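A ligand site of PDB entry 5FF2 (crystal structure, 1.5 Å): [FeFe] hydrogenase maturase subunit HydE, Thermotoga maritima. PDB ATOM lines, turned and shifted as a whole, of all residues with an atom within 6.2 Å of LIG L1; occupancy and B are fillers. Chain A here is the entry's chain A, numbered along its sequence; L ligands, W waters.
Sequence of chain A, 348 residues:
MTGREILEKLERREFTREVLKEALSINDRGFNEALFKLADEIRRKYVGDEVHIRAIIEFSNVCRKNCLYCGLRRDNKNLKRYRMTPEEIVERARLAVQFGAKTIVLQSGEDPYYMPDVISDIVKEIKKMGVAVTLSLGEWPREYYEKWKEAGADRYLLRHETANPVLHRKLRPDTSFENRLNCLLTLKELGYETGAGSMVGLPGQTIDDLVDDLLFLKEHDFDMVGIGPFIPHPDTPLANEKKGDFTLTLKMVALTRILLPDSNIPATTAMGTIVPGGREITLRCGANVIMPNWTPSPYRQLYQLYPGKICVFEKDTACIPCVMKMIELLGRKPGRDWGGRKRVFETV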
ATOM      1  N   VAL A  62      17.876  12.362  -4.866  1.00  0.00           N
ATOM      2  CA  VAL A  62      19.158  11.763  -5.274  1.00  0.00           C
ATOM      3  C   VAL A  62      20.257  12.471  -4.534  1.00  0.00           C
ATOM      4  O   VAL A  62      20.277  13.703  -4.481  1.00  0.00           O
ATOM      5  CB  VAL A  62      19.333  11.810  -6.785  1.00  0.00           C
ATOM      6  CG1 VAL A  62      20.742  11.377  -7.246  1.00  0.00           C
ATOM      7  CG2 VAL A  62      18.214  10.964  -7.449  1.00  0.00           C
ATOM      8  N   CYS A  63      21.185  11.707  -3.927  1.00  0.00           N
ATOM      9  CA  CYS A  63      22.337  12.323  -3.333  1.00  0.00           C
ATOM     10  C   CYS A  63      23.615  11.491  -3.566  1.00  0.00           C
ATOM     11  O   CYS A  63      23.622  10.271  -3.432  1.00  0.00           O
ATOM     12  CB  CYS A  63      22.168  12.564  -1.824  1.00  0.00           C
ATOM     13  SG  CYS A  63      23.381  13.703  -1.136  1.00  0.00           S
ATOM     14  N   ARG A  64      24.680  12.261  -3.817  1.00  0.00           N
ATOM     15  CA  ARG A  64      26.063  11.710  -3.994  1.00  0.00           C
ATOM     16  C   ARG A  64      26.791  11.542  -2.633  1.00  0.00           C
ATOM     17  O   ARG A  64      27.838  10.849  -2.599  1.00  0.00           O
ATOM     18  CB  ARG A  64      26.897  12.570  -4.898  1.00  0.00           C
ATOM     19  CG  ARG A  64      27.249  13.927  -4.316  1.00  0.00           C
ATOM     20  CD  ARG A  64      27.933  14.824  -5.333  1.00  0.00           C
ATOM     21  NE  ARG A  64      28.138  16.132  -4.773  1.00  0.00           N
ATOM     22  CZ  ARG A  64      28.967  17.049  -5.259  1.00  0.00           C
ATOM     23  NH1 ARG A  64      29.681  16.813  -6.350  1.00  0.00           N
ATOM     24  NH2 ARG A  64      29.116  18.186  -4.569  1.00  0.00           N
ATOM     25  N   LYS A  65      26.357  12.198  -1.582  1.00  0.00           N
ATOM     26  CA  LYS A  65      27.024  12.128  -0.319  1.00  0.00           C
ATOM     27  C   LYS A  65      26.426  11.016   0.577  1.00  0.00           C
ATOM     28  O   LYS A  65      25.400  10.435   0.263  1.00  0.00           O
ATOM     29  CB  LYS A  65      26.982  13.489   0.446  1.00  0.00           C
ATOM     30  CG  LYS A  65      28.035  14.463  -0.127  1.00  0.00           C
ATOM     31  CD  LYS A  65      28.119  15.742   0.653  1.00  0.00           C
ATOM     32  CE  LYS A  65      29.341  16.620   0.367  1.00  0.00           C
ATOM     33  NZ  LYS A  65      29.591  16.898  -1.043  1.00  0.00           N
ATOM     34  N   ASN A  66      27.098  10.761   1.705  1.00  0.00           N
ATOM     35  CA  ASN A  66      26.780   9.606   2.523  1.00  0.00           C
ATOM     36  C   ASN A  66      26.725   9.948   3.995  1.00  0.00           C
ATOM     37  O   ASN A  66      27.144   9.182   4.898  1.00  0.00           O
ATOM     38  CB  ASN A  66      27.855   8.478   2.311  1.00  0.00           C
ATOM     39  CG  ASN A  66      27.315   7.093   2.460  1.00  0.00           C
ATOM     40  OD1 ASN A  66      26.142   6.824   2.304  1.00  0.00           O
ATOM     41  ND2 ASN A  66      28.204   6.165   2.739  1.00  0.00           N
ATOM     42  N   CYS A  67      26.172  11.144   4.280  1.00  0.00           N
ATOM     43  CA  CYS A  67      26.117  11.613   5.676  1.00  0.00           C
ATOM     44  C   CYS A  67      25.426  10.555   6.572  1.00  0.00           C
ATOM     45  O   CYS A  67      24.433   9.980   6.208  1.00  0.00           O
ATOM     46  CB  CYS A  67      25.351  12.957   5.746  1.00  0.00           C
ATOM     47  SG  CYS A  67      25.999  14.232   4.639  1.00  0.00           S
ATOM     48  N   TYR A  69      23.756  10.462   9.284  1.00  0.00           N
ATOM     49  CA  TYR A  69      22.431  10.761   9.887  1.00  0.00           C
ATOM     50  C   TYR A  69      21.272  10.765   8.919  1.00  0.00           C
ATOM     51  O   TYR A  69      20.127  10.650   9.353  1.00  0.00           O
ATOM     52  CB  TYR A  69      22.476  12.109  10.641  1.00  0.00           C
ATOM     53  CG  TYR A  69      23.108  13.217   9.875  1.00  0.00           C
ATOM     54  CD1 TYR A  69      22.396  13.906   8.892  1.00  0.00           C
ATOM     55  CD2 TYR A  69      24.459  13.633  10.078  1.00  0.00           C
ATOM     56  CE1 TYR A  69      23.012  14.908   8.148  1.00  0.00           C
ATOM     57  CE2 TYR A  69      25.028  14.649   9.356  1.00  0.00           C
ATOM     58  CZ  TYR A  69      24.327  15.308   8.393  1.00  0.00           C
ATOM     59  OH  TYR A  69      24.943  16.271   7.697  1.00  0.00           O
ATOM     60  N   CYS A  70      21.543  10.857   7.598  1.00  0.00           N
ATOM     61  CA  CYS A  70      20.542  11.226   6.670  1.00  0.00           C
ATOM     62  C   CYS A  70      19.933  10.075   5.887  1.00  0.00           C
ATOM     63  O   CYS A  70      20.692   9.277   5.281  1.00  0.00           O
ATOM     64  CB  CYS A  70      21.125  12.194   5.660  1.00  0.00           C
ATOM     65  SG  CYS A  70      19.948  12.885   4.458  1.00  0.00           S
ATOM     66  N   GLY A  71      18.620   9.989   5.815  1.00  0.00           N
ATOM     67  CA  GLY A  71      17.957   8.958   5.061  1.00  0.00           C
ATOM     68  C   GLY A  71      18.183   8.963   3.560  1.00  0.00           C
ATOM     69  O   GLY A  71      17.975   7.954   2.879  1.00  0.00           O
ATOM     70  N   LEU A  72      18.625  10.130   3.016  1.00  0.00           N
ATOM     71  CA  LEU A  72      18.936  10.217   1.579  1.00  0.00           C
ATOM     72  C   LEU A  72      20.385   9.828   1.232  1.00  0.00           C
ATOM     73  O   LEU A  72      20.738   9.831   0.058  1.00  0.00           O
ATOM     74  CB  LEU A  72      18.712  11.658   1.068  1.00  0.00           C
ATOM     75  CG  LEU A  72      17.298  12.211   1.213  1.00  0.00           C
ATOM     76  CD1 LEU A  72      17.259  13.489   0.371  1.00  0.00           C
ATOM     77  CD2 LEU A  72      16.124  11.315   1.142  1.00  0.00           C
ATOM     78  N   ARG A  73      21.171   9.441   2.228  1.00  0.00           N
ATOM     79  CA  ARG A  73      22.568   9.030   1.988  1.00  0.00           C
ATOM     80  C   ARG A  73      22.682   8.032   0.845  1.00  0.00           C
ATOM     81  O   ARG A  73      21.861   7.168   0.691  1.00  0.00           O
ATOM     82  CB  ARG A  73      23.237   8.547   3.283  1.00  0.00           C
ATOM     83  CG  ARG A  73      22.646   7.239   3.816  1.00  0.00           C
ATOM     84  CD  ARG A  73      23.009   7.012   5.275  1.00  0.00           C
ATOM     85  NE  ARG A  73      24.450   7.110   5.486  1.00  0.00           N
ATOM     86  CZ  ARG A  73      25.351   6.135   5.428  1.00  0.00           C
ATOM     87  NH1 ARG A  73      25.001   4.895   5.159  1.00  0.00           N
ATOM     88  NH2 ARG A  73      26.628   6.420   5.648  1.00  0.00           N
ATOM     89  N   ARG A  74      23.790   8.160   0.102  1.00  0.00           N
ATOM     90  CA  ARG A  74      23.901   7.335  -1.111  1.00  0.00           C
ATOM     91  C   ARG A  74      23.828   5.821  -0.851  1.00  0.00           C
ATOM     92  O   ARG A  74      23.283   5.079  -1.713  1.00  0.00           O
ATOM     93  CB  ARG A  74      25.097   7.633  -1.952  1.00  0.00           C
ATOM     94  CG  ARG A  74      26.413   7.334  -1.349  1.00  0.00           C
ATOM     95  CD  ARG A  74      27.553   7.487  -2.362  1.00  0.00           C
ATOM     96  NE  ARG A  74      28.736   7.038  -1.625  1.00  0.00           N
ATOM     97  CZ  ARG A  74      29.531   7.814  -0.920  1.00  0.00           C
ATOM     98  NH1 ARG A  74      29.413   9.127  -0.959  1.00  0.00           N
ATOM     99  NH2 ARG A  74      30.515   7.252  -0.199  1.00  0.00           N
ATOM    100  N   SER A 108      17.209  19.883  -2.346  1.00  0.00           N
ATOM    101  CA  SER A 108      17.442  18.548  -2.871  1.00  0.00           C
ATOM    102  C   SER A 108      18.603  17.894  -2.141  1.00  0.00           C
ATOM    103  O   SER A 108      19.390  18.572  -1.466  1.00  0.00           O
ATOM    104  CB  SER A 108      17.756  18.578  -4.382  1.00  0.00           C
ATOM    105  OG  SER A 108      18.896  19.340  -4.643  1.00  0.00           O
ATOM    106  N   GLY A 109      18.725  16.581  -2.372  1.00  0.00           N
ATOM    107  CA  GLY A 109      19.987  15.935  -2.138  1.00  0.00           C
ATOM    108  C   GLY A 109      21.013  16.570  -3.094  1.00  0.00           C
ATOM    109  O   GLY A 109      20.672  17.339  -4.024  1.00  0.00           O
ATOM    110  N   GLU A 110      22.286  16.262  -2.878  1.00  0.00           N
ATOM    111  CA  GLU A 110      23.326  16.700  -3.801  1.00  0.00           C
ATOM    112  C   GLU A 110      23.275  15.847  -5.063  1.00  0.00           C
ATOM    113  O   GLU A 110      23.985  14.833  -5.223  1.00  0.00           O
ATOM    114  CB  GLU A 110      24.730  16.665  -3.171  1.00  0.00           C
ATOM    115  CG  GLU A 110      24.923  17.696  -2.085  1.00  0.00           C
ATOM    116  CD  GLU A 110      26.365  17.886  -1.701  1.00  0.00           C
ATOM    117  OE1 GLU A 110      27.262  17.330  -2.354  1.00  0.00           O
ATOM    118  OE2 GLU A 110      26.648  18.625  -0.725  1.00  0.00           O
ATOM    119  N   GLY A 138      23.217  22.014  -1.085  1.00  0.00           N
ATOM    120  CA  GLY A 138      24.492  21.411  -0.599  1.00  0.00           C
ATOM    121  C   GLY A 138      25.716  22.168  -1.050  1.00  0.00           C
ATOM    122  O   GLY A 138      25.667  23.364  -1.383  1.00  0.00           O
ATOM    123  N   GLU A 161      25.754  22.259  10.503  1.00  0.00           N
ATOM    124  CA  GLU A 161      25.491  20.904  11.054  1.00  0.00           C
ATOM    125  C   GLU A 161      26.055  20.727  12.489  1.00  0.00           C
ATOM    126  O   GLU A 161      25.288  20.431  13.395  1.00  0.00           O
ATOM    127  CB  GLU A 161      25.971  19.790  10.115  1.00  0.00           C
ATOM    128  CG  GLU A 161      25.567  19.978   8.668  1.00  0.00           C
ATOM    129  CD  GLU A 161      24.015  19.943   8.445  1.00  0.00           C
ATOM    130  OE1 GLU A 161      23.209  19.880   9.434  1.00  0.00           O
ATOM    131  OE2 GLU A 161      23.660  19.942   7.254  1.00  0.00           O
ATOM    132  N   ARG A 172      30.058  13.256   8.345  1.00  0.00           N
ATOM    133  CA  ARG A 172      29.978  13.677   6.943  1.00  0.00           C
ATOM    134  C   ARG A 172      31.283  13.311   6.216  1.00  0.00           C
ATOM    135  O   ARG A 172      32.113  14.181   5.933  1.00  0.00           O
ATOM    136  CB  ARG A 172      29.650  15.161   6.901  1.00  0.00           C
ATOM    137  CG  ARG A 172      28.432  15.505   7.747  1.00  0.00           C
ATOM    138  CD  ARG A 172      27.991  16.952   7.601  1.00  0.00           C
ATOM    139  NE  ARG A 172      27.419  17.119   6.244  1.00  0.00           N
ATOM    140  CZ  ARG A 172      27.930  17.822   5.248  1.00  0.00           C
ATOM    141  NH1 ARG A 172      28.905  18.597   5.408  1.00  0.00           N
ATOM    142  NH2 ARG A 172      27.364  17.681   4.056  1.00  0.00           N
ATOM    143  N   ARG A 180      32.641  23.116   4.515  1.00  0.00           N
ATOM    144  CA  ARG A 180      31.302  23.672   4.768  1.00  0.00           C
ATOM    145  C   ARG A 180      31.367  25.172   5.051  1.00  0.00           C
ATOM    146  O   ARG A 180      30.596  25.954   4.509  1.00  0.00           O
ATOM    147  CB  ARG A 180      30.666  22.935   5.943  1.00  0.00           C
ATOM    148  CG  ARG A 180      29.140  23.102   6.083  1.00  0.00           C
ATOM    149  CD  ARG A 180      28.456  22.195   5.124  1.00  0.00           C
ATOM    150  NE  ARG A 180      27.036  22.104   5.354  1.00  0.00           N
ATOM    151  CZ  ARG A 180      26.196  21.444   4.530  1.00  0.00           C
ATOM    152  NH1 ARG A 180      26.648  20.813   3.450  1.00  0.00           N
ATOM    153  NH2 ARG A 180      24.878  21.440   4.808  1.00  0.00           N
ATOM    154  N   TYR A 303      10.908  11.876   0.315  1.00  0.00           N
ATOM    155  CA  TYR A 303      11.924  12.802   0.808  1.00  0.00           C
ATOM    156  C   TYR A 303      12.003  12.716   2.275  1.00  0.00           C
ATOM    157  O   TYR A 303      11.417  13.475   2.997  1.00  0.00           O
ATOM    158  CB  TYR A 303      11.679  14.195   0.297  1.00  0.00           C
ATOM    159  CG  TYR A 303      12.878  15.111   0.425  1.00  0.00           C
ATOM    160  CD1 TYR A 303      13.827  15.199  -0.572  1.00  0.00           C
ATOM    161  CD2 TYR A 303      13.049  15.879   1.564  1.00  0.00           C
ATOM    162  CE1 TYR A 303      14.909  16.079  -0.486  1.00  0.00           C
ATOM    163  CE2 TYR A 303      14.084  16.755   1.684  1.00  0.00           C
ATOM    164  CZ  TYR A 303      15.035  16.817   0.670  1.00  0.00           C
ATOM    165  OH  TYR A 303      16.108  17.732   0.728  1.00  0.00           O
ATOM    166  N   LEU A 305      14.584  12.634   5.068  1.00  0.00           N
ATOM    167  CA  LEU A 305      15.838  12.900   5.737  1.00  0.00           C
ATOM    168  C   LEU A 305      15.779  12.144   7.039  1.00  0.00           C
ATOM    169  O   LEU A 305      16.737  11.551   7.424  1.00  0.00           O
ATOM    170  CB  LEU A 305      15.941  14.422   5.970  1.00  0.00           C
ATOM    171  CG  LEU A 305      15.871  15.318   4.753  1.00  0.00           C
ATOM    172  CD1 LEU A 305      15.834  16.780   5.267  1.00  0.00           C
ATOM    173  CD2 LEU A 305      17.053  15.085   3.874  1.00  0.00           C
HETATM  174 FE1  LIG L   1      21.454  14.110   3.236  1.00  0.00          FE
HETATM  175 FE2  LIG L   1      22.885  14.270   0.985  1.00  0.00          FE
HETATM  176 FE3  LIG L   1      24.063  14.702   3.433  1.00  0.00          FE
HETATM  177 FE4  LIG L   1      22.215  16.668   2.377  1.00  0.00          FE
HETATM  178  S1  LIG L   1      24.341  15.979   1.527  1.00  0.00           S
HETATM  179  S2  LIG L   1      22.391  15.742   4.526  1.00  0.00           S
HETATM  180  S3  LIG L   1      20.771  15.073   1.384  1.00  0.00           S
HETATM  181  S4  LIG L   1      23.209  12.731   2.639  1.00  0.00           S
HETATM  182  N1  LG2 L   2      21.712  18.269   0.791  1.00  0.00           N
HETATM  183  C1  LG2 L   2      21.530  19.574   1.370  1.00  0.00           C
HETATM  184  C2  LG2 L   2      20.108  19.818   1.713  1.00  0.00           C
HETATM  185  C3  LG2 L   2      19.136  18.727   2.118  1.00  0.00           C
HETATM  186  S1  LG2 L   2      19.459  18.220   3.786  1.00  0.00           S
HETATM  187  C4  LG2 L   2      22.433  19.747   2.513  1.00  0.00           C
HETATM  188  O1  LG2 L   2      22.593  20.939   2.835  1.00  0.00           O
HETATM  189  O2  LG2 L   2      22.949  18.757   3.095  1.00  0.00           O
HETATM  190  C5  LG2 L   2      18.698  19.478   4.797  1.00  0.00           C
HETATM  191  C6  LG2 L   2      19.071  19.393   6.256  1.00  0.00           C
HETATM  192  O3  LG2 L   2      18.326  18.337   6.916  1.00  0.00           O
HETATM  193  C7  LG2 L   2      20.493  19.104   6.708  1.00  0.00           C
HETATM  194  O4  LG2 L   2      21.239  20.333   6.692  1.00  0.00           O
HETATM  195  C8  LG2 L   2      20.324  18.491   8.101  1.00  0.00           C
HETATM  196  O5  LG2 L   2      20.642  19.384   9.189  1.00  0.00           O
HETATM  197  C9  LG2 L   2      18.881  17.988   8.135  1.00  0.00           C
HETATM  198  N2  LG2 L   2      18.800  16.579   8.378  1.00  0.00           N
HETATM  199  C10 LG2 L   2      19.299  15.544   7.607  1.00  0.00           C
HETATM  200  N3  LG2 L   2      19.131  14.361   8.224  1.00  0.00           N
HETATM  201  C11 LG2 L   2      18.559  14.628   9.410  1.00  0.00           C
HETATM  202  C12 LG2 L   2      18.072  13.819  10.490  1.00  0.00           C
HETATM  203  N4  LG2 L   2      18.239  12.496  10.523  1.00  0.00           N
HETATM  204  N5  LG2 L   2      17.497  14.436  11.528  1.00  0.00           N
HETATM  205  C13 LG2 L   2      17.287  15.784  11.500  1.00  0.00           C
HETATM  206  N6  LG2 L   2      17.692  16.541  10.536  1.00  0.00           N
HETATM  207  C14 LG2 L   2      18.302  16.054   9.472  1.00  0.00           C
HETATM  208  O   HOH W   1      24.490  17.942   5.567  1.00  0.00           O
HETATM  209  O   HOH W   2      25.579  19.029   1.703  1.00  0.00           O
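SG of Cys 63 lies close to N of Lys 65.
The backbone NH (N) of Leu 72 sits close to the side-chain sulfur (SG) of Cys 70 (3.4 Å).
O of Cys 67 lies within hydrogen-bond range of NE of Arg 73 (3.0 Å).
The side-chain sulfur (SG) of Cys 67 lies close to the guanidinium group (NE) of Arg 172.
OH of Tyr 69 is in hydrogen-bond range of NE of Arg 172, at 3.0 Å.
NZ of Lys 65 is in salt-bridge range of OE1 of Glu 110.
The backbone carbonyl oxygen (O) of Lys 65 is in hydrogen-bond range of the backbone NH (N) of Arg 74.
O of Asn 66 sits at hydrogen-bond distance from NH2 of Arg 73.
Lys 65 touches LIG L1 (CB to S1, 3.8 Å).
Tyr 69 touches LIG L1.
CD1 of Leu 72 touches S3 of LIG L1 (3.98 Å).
Arg 73 touches LIG L1 (CA to S4, 3.8 Å).
CA of Gly 109 touches S3 of LIG L1, at 3.7 Å.
Hydrophobic or aromatic side chains that line LIG L1: Tyr 69 and Leu 72.
The nearest printed residue that does not touch LIG L1 is Glu 110 (4.04 Å).
The side-chain sulfur (SG) of Cys 63 binds an iron atom (FE2) of LIG L1, at 2.3 Å.
An iron atom (FE1) of LIG L1 is bound by the side-chain sulfur of Cys 70.
The backbone NH (N) of Cys 67 lies close to a sulfur (S4) of LIG L1, 3.7 Å away.
FE3 of LIG L1 is bound by SG of Cys 67 (2.3 Å).
The backbone carbonyl oxygen of Tyr 69 lies within hydrogen-bond range of a nitrogen (N4) of LG2 L2 (2.9 Å).
A nitrogen (N1) of LG2 L2 sits close to the backbone carbonyl oxygen of Ser 108, at 3.3 Å.
The side-chain carboxylate (OE2) of Glu 161 sits at hydrogen-bond distance from an oxygen (O4) of LG2 L2, at 2.5 Å.
An oxygen (O1) of LG2 L2 is in salt-bridge range of the guanidinium group of Arg 180, 3.1 Å away.
Water W1 lies within hydrogen-bond range of OE2 of Glu 161, OH of Tyr 69, NE of Arg 172 and S2 of LIG L1.
Water W2 lies within hydrogen-bond range of the side-chain carboxylate (OE2) of Glu 110, the guanidinium group (NH1) of Arg 180, the guanidinium group (NH2) of Arg 172 and a sulfur (S1) of LIG L1.
A nitrogen (N1) of LG2 L2 is bound to an iron atom (FE4) of LIG L1, 2.3 Å away.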
